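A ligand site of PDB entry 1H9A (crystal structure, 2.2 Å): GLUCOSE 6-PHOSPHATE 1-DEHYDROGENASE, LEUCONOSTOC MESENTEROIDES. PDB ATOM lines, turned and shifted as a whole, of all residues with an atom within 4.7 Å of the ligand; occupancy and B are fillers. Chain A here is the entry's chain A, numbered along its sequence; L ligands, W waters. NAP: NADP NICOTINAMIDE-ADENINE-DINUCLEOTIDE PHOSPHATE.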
ATOM      1  N   GLY A  12     -17.150  18.879 -24.457  1.00  0.00           N
ATOM      2  CA  GLY A  12     -16.542  19.969 -23.718  1.00  0.00           C
ATOM      3  C   GLY A  12     -17.338  21.226 -24.022  1.00  0.00           C
ATOM      4  O   GLY A  12     -16.798  22.339 -24.026  1.00  0.00           O
ATOM      5  N   GLY A  13     -18.638  21.041 -24.226  1.00  0.00           N
ATOM      6  CA  GLY A  13     -19.530  22.128 -24.562  1.00  0.00           C
ATOM      7  C   GLY A  13     -19.663  23.240 -23.545  1.00  0.00           C
ATOM      8  O   GLY A  13     -20.158  24.319 -23.861  1.00  0.00           O
ATOM      9  N   THR A  14     -19.259  22.992 -22.315  1.00  0.00           N
ATOM     10  CA  THR A  14     -19.353  24.018 -21.286  1.00  0.00           C
ATOM     11  C   THR A  14     -17.993  24.665 -21.056  1.00  0.00           C
ATOM     12  O   THR A  14     -17.846  25.553 -20.218  1.00  0.00           O
ATOM     13  CB  THR A  14     -19.882  23.429 -19.980  1.00  0.00           C
ATOM     14  OG1 THR A  14     -19.074  22.313 -19.622  1.00  0.00           O
ATOM     15  CG2 THR A  14     -21.317  22.964 -20.158  1.00  0.00           C
ATOM     16  N   GLY A  15     -17.010  24.216 -21.827  1.00  0.00           N
ATOM     17  CA  GLY A  15     -15.647  24.715 -21.698  1.00  0.00           C
ATOM     18  C   GLY A  15     -15.423  26.158 -22.079  1.00  0.00           C
ATOM     19  O   GLY A  15     -16.238  26.782 -22.753  1.00  0.00           O
ATOM     20  N   ASP A  16     -14.269  26.665 -21.663  1.00  0.00           N
ATOM     21  CA  ASP A  16     -13.872  28.039 -21.935  1.00  0.00           C
ATOM     22  C   ASP A  16     -13.771  28.321 -23.431  1.00  0.00           C
ATOM     23  O   ASP A  16     -14.260  29.334 -23.920  1.00  0.00           O
ATOM     24  CB  ASP A  16     -12.532  28.321 -21.227  1.00  0.00           C
ATOM     25  CG  ASP A  16     -11.959  29.687 -21.571  1.00  0.00           C
ATOM     26  OD1 ASP A  16     -12.506  30.701 -21.074  1.00  0.00           O
ATOM     27  OD2 ASP A  16     -10.973  29.740 -22.347  1.00  0.00           O
ATOM     28  N   LEU A  17     -13.158  27.388 -24.170  1.00  0.00           N
ATOM     29  CA  LEU A  17     -12.996  27.532 -25.618  1.00  0.00           C
ATOM     30  C   LEU A  17     -14.342  27.524 -26.336  1.00  0.00           C
ATOM     31  O   LEU A  17     -14.549  28.289 -27.284  1.00  0.00           O
ATOM     32  CB  LEU A  17     -12.108  26.419 -26.179  1.00  0.00           C
ATOM     33  CG  LEU A  17     -11.854  26.479 -27.689  1.00  0.00           C
ATOM     34  CD1 LEU A  17     -10.943  27.655 -27.998  1.00  0.00           C
ATOM     35  CD2 LEU A  17     -11.251  25.177 -28.188  1.00  0.00           C
ATOM     36  N   ALA A  18     -15.251  26.666 -25.901  1.00  0.00           N
ATOM     37  CA  ALA A  18     -16.565  26.562 -26.500  1.00  0.00           C
ATOM     38  C   ALA A  18     -17.308  27.885 -26.412  1.00  0.00           C
ATOM     39  O   ALA A  18     -17.765  28.413 -27.422  1.00  0.00           O
ATOM     40  CB  ALA A  18     -17.359  25.448 -25.852  1.00  0.00           C
ATOM     41  N   ARG A  20     -16.051  30.969 -25.546  1.00  0.00           N
ATOM     42  CA  ARG A  20     -15.298  32.141 -26.000  1.00  0.00           C
ATOM     43  C   ARG A  20     -15.064  32.160 -27.513  1.00  0.00           C
ATOM     44  O   ARG A  20     -15.089  33.219 -28.131  1.00  0.00           O
ATOM     45  CB  ARG A  20     -13.940  32.215 -25.292  1.00  0.00           C
ATOM     46  CG  ARG A  20     -13.907  33.063 -24.030  1.00  0.00           C
ATOM     47  CD  ARG A  20     -12.512  33.081 -23.376  1.00  0.00           C
ATOM     48  NE  ARG A  20     -11.477  33.729 -24.197  1.00  0.00           N
ATOM     49  CZ  ARG A  20     -10.653  33.100 -25.039  1.00  0.00           C
ATOM     50  NH1 ARG A  20     -10.738  31.774 -25.208  1.00  0.00           N
ATOM     51  NH2 ARG A  20      -9.722  33.786 -25.708  1.00  0.00           N
ATOM     52  N   ALA A  45     -21.102  17.535 -21.821  1.00  0.00           N
ATOM     53  CA  ALA A  45     -20.085  17.583 -20.753  1.00  0.00           C
ATOM     54  C   ALA A  45     -20.689  16.817 -19.562  1.00  0.00           C
ATOM     55  O   ALA A  45     -21.810  16.313 -19.654  1.00  0.00           O
ATOM     56  CB  ALA A  45     -19.787  19.018 -20.367  1.00  0.00           C
ATOM     57  N   ARG A  46     -19.965  16.725 -18.456  1.00  0.00           N
ATOM     58  CA  ARG A  46     -20.500  16.010 -17.295  1.00  0.00           C
ATOM     59  C   ARG A  46     -21.548  16.810 -16.556  1.00  0.00           C
ATOM     60  O   ARG A  46     -22.526  16.244 -16.057  1.00  0.00           O
ATOM     61  CB  ARG A  46     -19.389  15.630 -16.322  1.00  0.00           C
ATOM     62  CG  ARG A  46     -18.402  14.581 -16.809  1.00  0.00           C
ATOM     63  CD  ARG A  46     -17.222  14.539 -15.851  1.00  0.00           C
ATOM     64  NE  ARG A  46     -16.740  15.895 -15.578  1.00  0.00           N
ATOM     65  CZ  ARG A  46     -15.552  16.200 -15.074  1.00  0.00           C
ATOM     66  NH1 ARG A  46     -14.677  15.234 -14.762  1.00  0.00           N
ATOM     67  NH2 ARG A  46     -15.231  17.476 -14.858  1.00  0.00           N
ATOM     68  N   GLN A  47     -21.350  18.123 -16.481  1.00  0.00           N
ATOM     69  CA  GLN A  47     -22.274  19.021 -15.789  1.00  0.00           C
ATOM     70  C   GLN A  47     -23.744  18.750 -16.175  1.00  0.00           C
ATOM     71  O   GLN A  47     -24.099  18.757 -17.357  1.00  0.00           O
ATOM     72  CB  GLN A  47     -21.914  20.466 -16.091  1.00  0.00           C
ATOM     73  CG  GLN A  47     -22.497  21.453 -15.101  1.00  0.00           C
ATOM     74  CD  GLN A  47     -22.309  22.905 -15.516  1.00  0.00           C
ATOM     75  OE1 GLN A  47     -23.037  23.789 -15.053  1.00  0.00           O
ATOM     76  NE2 GLN A  47     -21.342  23.159 -16.382  1.00  0.00           N
ATOM     77  N   HIS A  84     -22.898  13.852 -19.957  1.00  0.00           N
ATOM     78  CA  HIS A  84     -22.267  12.611 -20.380  1.00  0.00           C
ATOM     79  C   HIS A  84     -20.789  12.538 -19.988  1.00  0.00           C
ATOM     80  O   HIS A  84     -20.049  13.510 -20.139  1.00  0.00           O
ATOM     81  CB  HIS A  84     -22.405  12.533 -21.906  1.00  0.00           C
ATOM     82  CG  HIS A  84     -21.583  11.459 -22.536  1.00  0.00           C
ATOM     83  ND1 HIS A  84     -21.804  10.122 -22.309  1.00  0.00           N
ATOM     84  CD2 HIS A  84     -20.556  11.520 -23.414  1.00  0.00           C
ATOM     85  CE1 HIS A  84     -20.941   9.401 -23.008  1.00  0.00           C
ATOM     86  NE2 HIS A  84     -20.162  10.232 -23.684  1.00  0.00           N
ATOM     87  N   ASP A  85     -20.360  11.381 -19.472  1.00  0.00           N
ATOM     88  CA  ASP A  85     -18.957  11.185 -19.092  1.00  0.00           C
ATOM     89  C   ASP A  85     -18.297  10.431 -20.238  1.00  0.00           C
ATOM     90  O   ASP A  85     -18.751   9.338 -20.591  1.00  0.00           O
ATOM     91  CB  ASP A  85     -18.836  10.362 -17.799  1.00  0.00           C
ATOM     92  CG  ASP A  85     -17.429  10.405 -17.197  1.00  0.00           C
ATOM     93  OD1 ASP A  85     -16.438  10.261 -17.941  1.00  0.00           O
ATOM     94  OD2 ASP A  85     -17.311  10.587 -15.964  1.00  0.00           O
ATOM     95  N   VAL A  86     -17.228  10.997 -20.804  1.00  0.00           N
ATOM     96  CA  VAL A  86     -16.549  10.365 -21.938  1.00  0.00           C
ATOM     97  C   VAL A  86     -15.823   9.059 -21.646  1.00  0.00           C
ATOM     98  O   VAL A  86     -15.451   8.333 -22.580  1.00  0.00           O
ATOM     99  CB  VAL A  86     -15.569  11.345 -22.612  1.00  0.00           C
ATOM    100  CG1 VAL A  86     -16.332  12.526 -23.196  1.00  0.00           C
ATOM    101  CG2 VAL A  86     -14.512  11.812 -21.625  1.00  0.00           C
ATOM    102  N   SER A 117     -13.334  19.377 -27.676  1.00  0.00           N
ATOM    103  CA  SER A 117     -12.783  20.495 -26.928  1.00  0.00           C
ATOM    104  C   SER A 117     -12.605  20.032 -25.468  1.00  0.00           C
ATOM    105  O   SER A 117     -13.095  20.659 -24.523  1.00  0.00           O
ATOM    106  CB  SER A 117     -13.717  21.706 -27.008  1.00  0.00           C
ATOM    107  OG  SER A 117     -13.046  22.903 -26.637  1.00  0.00           O
ATOM    108  N   VAL A 118     -11.892  18.931 -25.317  1.00  0.00           N
ATOM    109  CA  VAL A 118     -11.628  18.337 -24.013  1.00  0.00           C
ATOM    110  C   VAL A 118     -10.122  18.134 -23.820  1.00  0.00           C
ATOM    111  O   VAL A 118      -9.335  18.480 -24.693  1.00  0.00           O
ATOM    112  CB  VAL A 118     -12.374  16.968 -23.857  1.00  0.00           C
ATOM    113  CG1 VAL A 118     -13.872  17.183 -23.907  1.00  0.00           C
ATOM    114  CG2 VAL A 118     -11.942  16.002 -24.964  1.00  0.00           C
ATOM    115  N   ALA A 119      -9.740  17.558 -22.683  1.00  0.00           N
ATOM    116  CA  ALA A 119      -8.330  17.283 -22.391  1.00  0.00           C
ATOM    117  C   ALA A 119      -7.810  16.255 -23.384  1.00  0.00           C
ATOM    118  O   ALA A 119      -8.507  15.285 -23.712  1.00  0.00           O
ATOM    119  CB  ALA A 119      -8.158  16.777 -20.965  1.00  0.00           C
ATOM    120  N   PRO A 120      -6.575  16.420 -23.847  1.00  0.00           N
ATOM    121  CA  PRO A 120      -5.938  15.521 -24.813  1.00  0.00           C
ATOM    122  C   PRO A 120      -5.999  14.024 -24.487  1.00  0.00           C
ATOM    123  O   PRO A 120      -6.119  13.208 -25.392  1.00  0.00           O
ATOM    124  CB  PRO A 120      -4.492  16.022 -24.831  1.00  0.00           C
ATOM    125  CG  PRO A 120      -4.664  17.482 -24.604  1.00  0.00           C
ATOM    126  CD  PRO A 120      -5.661  17.508 -23.482  1.00  0.00           C
ATOM    127  N   PHE A 122      -8.302  12.290 -23.515  1.00  0.00           N
ATOM    128  CA  PHE A 122      -9.588  11.699 -23.900  1.00  0.00           C
ATOM    129  C   PHE A 122      -9.737  11.457 -25.400  1.00  0.00           C
ATOM    130  O   PHE A 122     -10.594  10.662 -25.807  1.00  0.00           O
ATOM    131  CB  PHE A 122     -10.720  12.591 -23.419  1.00  0.00           C
ATOM    132  CG  PHE A 122     -10.740  12.791 -21.928  1.00  0.00           C
ATOM    133  CD1 PHE A 122     -10.761  11.696 -21.077  1.00  0.00           C
ATOM    134  CD2 PHE A 122     -10.748  14.072 -21.388  1.00  0.00           C
ATOM    135  CE1 PHE A 122     -10.796  11.865 -19.698  1.00  0.00           C
ATOM    136  CE2 PHE A 122     -10.783  14.260 -20.003  1.00  0.00           C
ATOM    137  CZ  PHE A 122     -10.797  13.158 -19.162  1.00  0.00           C
ATOM    138  N   PHE A 123      -8.899  12.106 -26.202  1.00  0.00           N
ATOM    139  CA  PHE A 123      -8.958  11.999 -27.658  1.00  0.00           C
ATOM    140  C   PHE A 123      -9.161  10.611 -28.239  1.00  0.00           C
ATOM    141  O   PHE A 123     -10.106  10.393 -28.996  1.00  0.00           O
ATOM    142  CB  PHE A 123      -7.737  12.663 -28.302  1.00  0.00           C
ATOM    143  CG  PHE A 123      -7.712  14.145 -28.175  1.00  0.00           C
ATOM    144  CD1 PHE A 123      -8.840  14.845 -27.749  1.00  0.00           C
ATOM    145  CD2 PHE A 123      -6.565  14.863 -28.501  1.00  0.00           C
ATOM    146  CE1 PHE A 123      -8.820  16.230 -27.643  1.00  0.00           C
ATOM    147  CE2 PHE A 123      -6.539  16.259 -28.400  1.00  0.00           C
ATOM    148  CZ  PHE A 123      -7.666  16.936 -27.965  1.00  0.00           C
ATOM    149  N   GLU A 147      -8.525  18.984 -31.168  1.00  0.00           N
ATOM    150  CA  GLU A 147      -7.838  20.169 -30.683  1.00  0.00           C
ATOM    151  C   GLU A 147      -6.370  19.827 -30.441  1.00  0.00           C
ATOM    152  O   GLU A 147      -5.970  18.671 -30.520  1.00  0.00           O
ATOM    153  CB  GLU A 147      -8.477  20.673 -29.388  1.00  0.00           C
ATOM    154  CG  GLU A 147      -9.376  21.890 -29.562  1.00  0.00           C
ATOM    155  CD  GLU A 147      -8.633  23.123 -30.079  1.00  0.00           C
ATOM    156  OE1 GLU A 147      -7.430  23.282 -29.793  1.00  0.00           O
ATOM    157  OE2 GLU A 147      -9.276  23.940 -30.768  1.00  0.00           O
ATOM    158  N   LYS A 148      -5.563  20.851 -30.188  1.00  0.00           N
ATOM    159  CA  LYS A 148      -4.140  20.631 -29.940  1.00  0.00           C
ATOM    160  C   LYS A 148      -3.919  20.172 -28.494  1.00  0.00           C
ATOM    161  O   LYS A 148      -4.694  20.517 -27.602  1.00  0.00           O
ATOM    162  CB  LYS A 148      -3.330  21.895 -30.237  1.00  0.00           C
ATOM    163  CG  LYS A 148      -3.577  23.039 -29.268  1.00  0.00           C
ATOM    164  CD  LYS A 148      -2.306  23.874 -29.085  1.00  0.00           C
ATOM    165  CE  LYS A 148      -2.385  24.683 -27.802  1.00  0.00           C
ATOM    166  NZ  LYS A 148      -2.775  23.822 -26.628  1.00  0.00           N
ATOM    167  N   TYR A 415     -10.999  30.386 -36.146  1.00  0.00           N
ATOM    168  CA  TYR A 415     -11.903  29.291 -35.793  1.00  0.00           C
ATOM    169  C   TYR A 415     -13.115  29.186 -36.710  1.00  0.00           C
ATOM    170  O   TYR A 415     -13.547  28.073 -37.032  1.00  0.00           O
ATOM    171  CB  TYR A 415     -12.316  29.334 -34.324  1.00  0.00           C
ATOM    172  CG  TYR A 415     -11.326  28.616 -33.415  1.00  0.00           C
ATOM    173  CD1 TYR A 415     -11.315  27.214 -33.350  1.00  0.00           C
ATOM    174  CD2 TYR A 415     -10.398  29.323 -32.659  1.00  0.00           C
ATOM    175  CE1 TYR A 415     -10.391  26.543 -32.537  1.00  0.00           C
ATOM    176  CE2 TYR A 415      -9.467  28.654 -31.853  1.00  0.00           C
ATOM    177  CZ  TYR A 415      -9.471  27.275 -31.795  1.00  0.00           C
ATOM    178  OH  TYR A 415      -8.562  26.636 -30.987  1.00  0.00           O
HETATM  179  PA  NAP L   1     -11.782  23.599 -20.149  1.00  0.00           P
HETATM  180  O1A NAP L   1     -11.065  22.854 -19.088  1.00  0.00           O
HETATM  181  O2A NAP L   1     -12.411  24.835 -19.639  1.00  0.00           O
HETATM  182  O5B NAP L   1     -13.039  22.678 -20.503  1.00  0.00           O
HETATM  183  C5B NAP L   1     -13.041  21.255 -20.400  1.00  0.00           C
HETATM  184  C4B NAP L   1     -14.392  20.713 -20.851  1.00  0.00           C
HETATM  185  O4B NAP L   1     -14.359  19.257 -20.809  1.00  0.00           O
HETATM  186  C3B NAP L   1     -15.486  21.138 -19.893  1.00  0.00           C
HETATM  187  O3B NAP L   1     -16.643  21.515 -20.638  1.00  0.00           O
HETATM  188  C2B NAP L   1     -15.737  19.910 -19.068  1.00  0.00           C
HETATM  189  O2B NAP L   1     -17.082  19.876 -18.632  1.00  0.00           O
HETATM  190  C1B NAP L   1     -15.456  18.792 -20.052  1.00  0.00           C
HETATM  191  N9A NAP L   1     -15.143  17.501 -19.403  1.00  0.00           N
HETATM  192  C8A NAP L   1     -14.205  17.253 -18.433  1.00  0.00           C
HETATM  193  N7A NAP L   1     -14.003  15.970 -18.184  1.00  0.00           N
HETATM  194  C5A NAP L   1     -14.939  15.349 -18.952  1.00  0.00           C
HETATM  195  C6A NAP L   1     -15.249  14.016 -19.001  1.00  0.00           C
HETATM  196  N6A NAP L   1     -14.646  13.196 -18.091  1.00  0.00           N
HETATM  197  N1A NAP L   1     -16.251  13.696 -19.844  1.00  0.00           N
HETATM  198  C2A NAP L   1     -16.882  14.641 -20.541  1.00  0.00           C
HETATM  199  N3A NAP L   1     -16.615  15.927 -20.622  1.00  0.00           N
HETATM  200  C4A NAP L   1     -15.642  16.235 -19.738  1.00  0.00           C
HETATM  201  O3  NAP L   1     -10.877  23.841 -21.414  1.00  0.00           O
HETATM  202  PN  NAP L   1     -10.764  24.605 -22.780  1.00  0.00           P
HETATM  203  O1N NAP L   1      -9.999  25.872 -22.685  1.00  0.00           O
HETATM  204  O2N NAP L   1     -12.100  24.864 -23.378  1.00  0.00           O
HETATM  205  O5D NAP L   1      -9.954  23.788 -23.910  1.00  0.00           O
HETATM  206  C5D NAP L   1     -10.130  22.384 -24.106  1.00  0.00           C
HETATM  207  C4D NAP L   1      -9.349  21.874 -25.332  1.00  0.00           C
HETATM  208  O4D NAP L   1      -9.096  22.963 -26.256  1.00  0.00           O
HETATM  209  C3D NAP L   1      -7.987  21.337 -24.923  1.00  0.00           C
HETATM  210  O3D NAP L   1      -7.566  20.308 -25.812  1.00  0.00           O
HETATM  211  C2D NAP L   1      -7.090  22.535 -25.093  1.00  0.00           C
HETATM  212  O2D NAP L   1      -5.768  22.090 -25.378  1.00  0.00           O
HETATM  213  C1D NAP L   1      -7.701  23.189 -26.336  1.00  0.00           C
HETATM  214  N1N NAP L   1      -7.325  24.620 -26.482  1.00  0.00           N
HETATM  215  C2N NAP L   1      -7.953  25.560 -25.769  1.00  0.00           C
HETATM  216  C3N NAP L   1      -7.687  26.879 -25.929  1.00  0.00           C
HETATM  217  C7N NAP L   1      -8.243  28.086 -25.237  1.00  0.00           C
HETATM  218  O7N NAP L   1      -7.834  29.204 -25.560  1.00  0.00           O
HETATM  219  N7N NAP L   1      -9.381  27.826 -24.546  1.00  0.00           N
HETATM  220  C4N NAP L   1      -6.753  27.230 -26.884  1.00  0.00           C
HETATM  221  C5N NAP L   1      -6.083  26.269 -27.589  1.00  0.00           C
HETATM  222  C6N NAP L   1      -6.375  24.964 -27.336  1.00  0.00           C
HETATM  223  P2B NAP L   1     -17.394  19.139 -17.269  1.00  0.00           P
HETATM  224  O1X NAP L   1     -16.287  19.506 -16.363  1.00  0.00           O
HETATM  225  O2X NAP L   1     -17.415  17.703 -17.596  1.00  0.00           O
HETATM  226  O3X NAP L   1     -18.716  19.656 -16.832  1.00  0.00           O
HETATM  227  O   HOH W   1     -14.293  24.210 -24.551  1.00  0.00           O
HETATM  228  O   HOH W   2     -17.432  16.313 -23.460  1.00  0.00           O
HETATM  229  O   HOH W   3     -11.894  15.424 -16.343  1.00  0.00           O
HETATM  230  O   HOH W   4     -19.063  22.112 -16.974  1.00  0.00           O
HETATM  231  O   HOH W   5     -11.710  17.951 -20.614  1.00  0.00           O
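The side-chain hydroxyl (OH) of Tyr 415 lies within hydrogen-bond range of the side-chain carboxylate (OE2) of Glu 147 (2.8 Å). OD2 of Asp 16 is in salt-bridge range of NH1 of Arg 20, at 3.5 Å. The backbone NH (N) of His 84 lies within hydrogen-bond range of the backbone carbonyl oxygen (O) of Ala 45, at 2.7 Å.
Residues that only touch the ligand: Arg 20 (3.9 Å), Ala 45 (3.3 Å), His 84 (3.4 Å), Ser 117 (3.5 Å), Phe 122 (3.995 Å) and Glu 147 (3.2 Å). The nearest printed residue that does not touch the ligand is Phe 123 (4.002 Å).
The backbone NH (N) of Arg 46 is in hydrogen-bond range of an oxygen (O2X) of the ligand. The guanidinium group (NH2) of Arg 46 is in salt-bridge range of an oxygen (O1X) of the ligand, at 2.7 Å. The backbone NH (N) of Thr 14 lies within hydrogen-bond range of an oxygen (O3B) of the ligand (3.4 Å). An oxygen (O3B) of the ligand sits at hydrogen-bond distance from the side-chain hydroxyl (OG1) of Thr 14 (2.8 Å). O of Val 118 lies within hydrogen-bond range of O3D of the ligand (2.8 Å). The backbone NH (N) of Leu 17 sits at hydrogen-bond distance from an oxygen (O2N) of the ligand, at 2.8 Å. The backbone carbonyl oxygen (O) of Lys 148 sits at hydrogen-bond distance from an oxygen (O2D) of the ligand (2.9 Å). The backbone NH (N) of Gly 15 sits at hydrogen-bond distance from an oxygen (O3B) of the ligand. The backbone NH of Val 86 is in hydrogen-bond range of a nitrogen (N1A) of the ligand (3.0 Å). The backbone NH (N) of Gln 47 is in hydrogen-bond range of an oxygen (O3X) of the ligand. An oxygen (O2N) of the ligand is in hydrogen-bond range of the backbone NH (N) of Asp 16, at 3.3 Å. The side-chain carboxylate (OD2) of Asp 16 lies within hydrogen-bond range of a nitrogen (N7N) of the ligand, at 3.3 Å. N6A of the ligand is in hydrogen-bond range of OD1 of Asp 85, at 3.4 Å. The backbone carbonyl oxygen (O) of Gly 12 sits close to an oxygen (O3B) of the ligand (3.5 Å).
Water W4 lies within hydrogen-bond range of O3X of the ligand, NE2 of Gln 47 and OG1 of Thr 14. Water W1 lies within hydrogen-bond range of an oxygen (O2N) of the ligand, the side-chain hydroxyl (OG) of Ser 117, the backbone NH (N) of Ala 18, the backbone carbonyl oxygen (O) of Gly 12 and the backbone NH (N) of Leu 17. Water W3 bridges N7A of the ligand and NH1 of Arg 46. Water W5 bridges the backbone NH of Ala 119 and an oxygen (O4B) of the ligand. Water W2 lies within hydrogen-bond range of the backbone NH (N) of Gly 12 (2.8 Å) and a nitrogen (N3A) of the ligand (3.0 Å).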
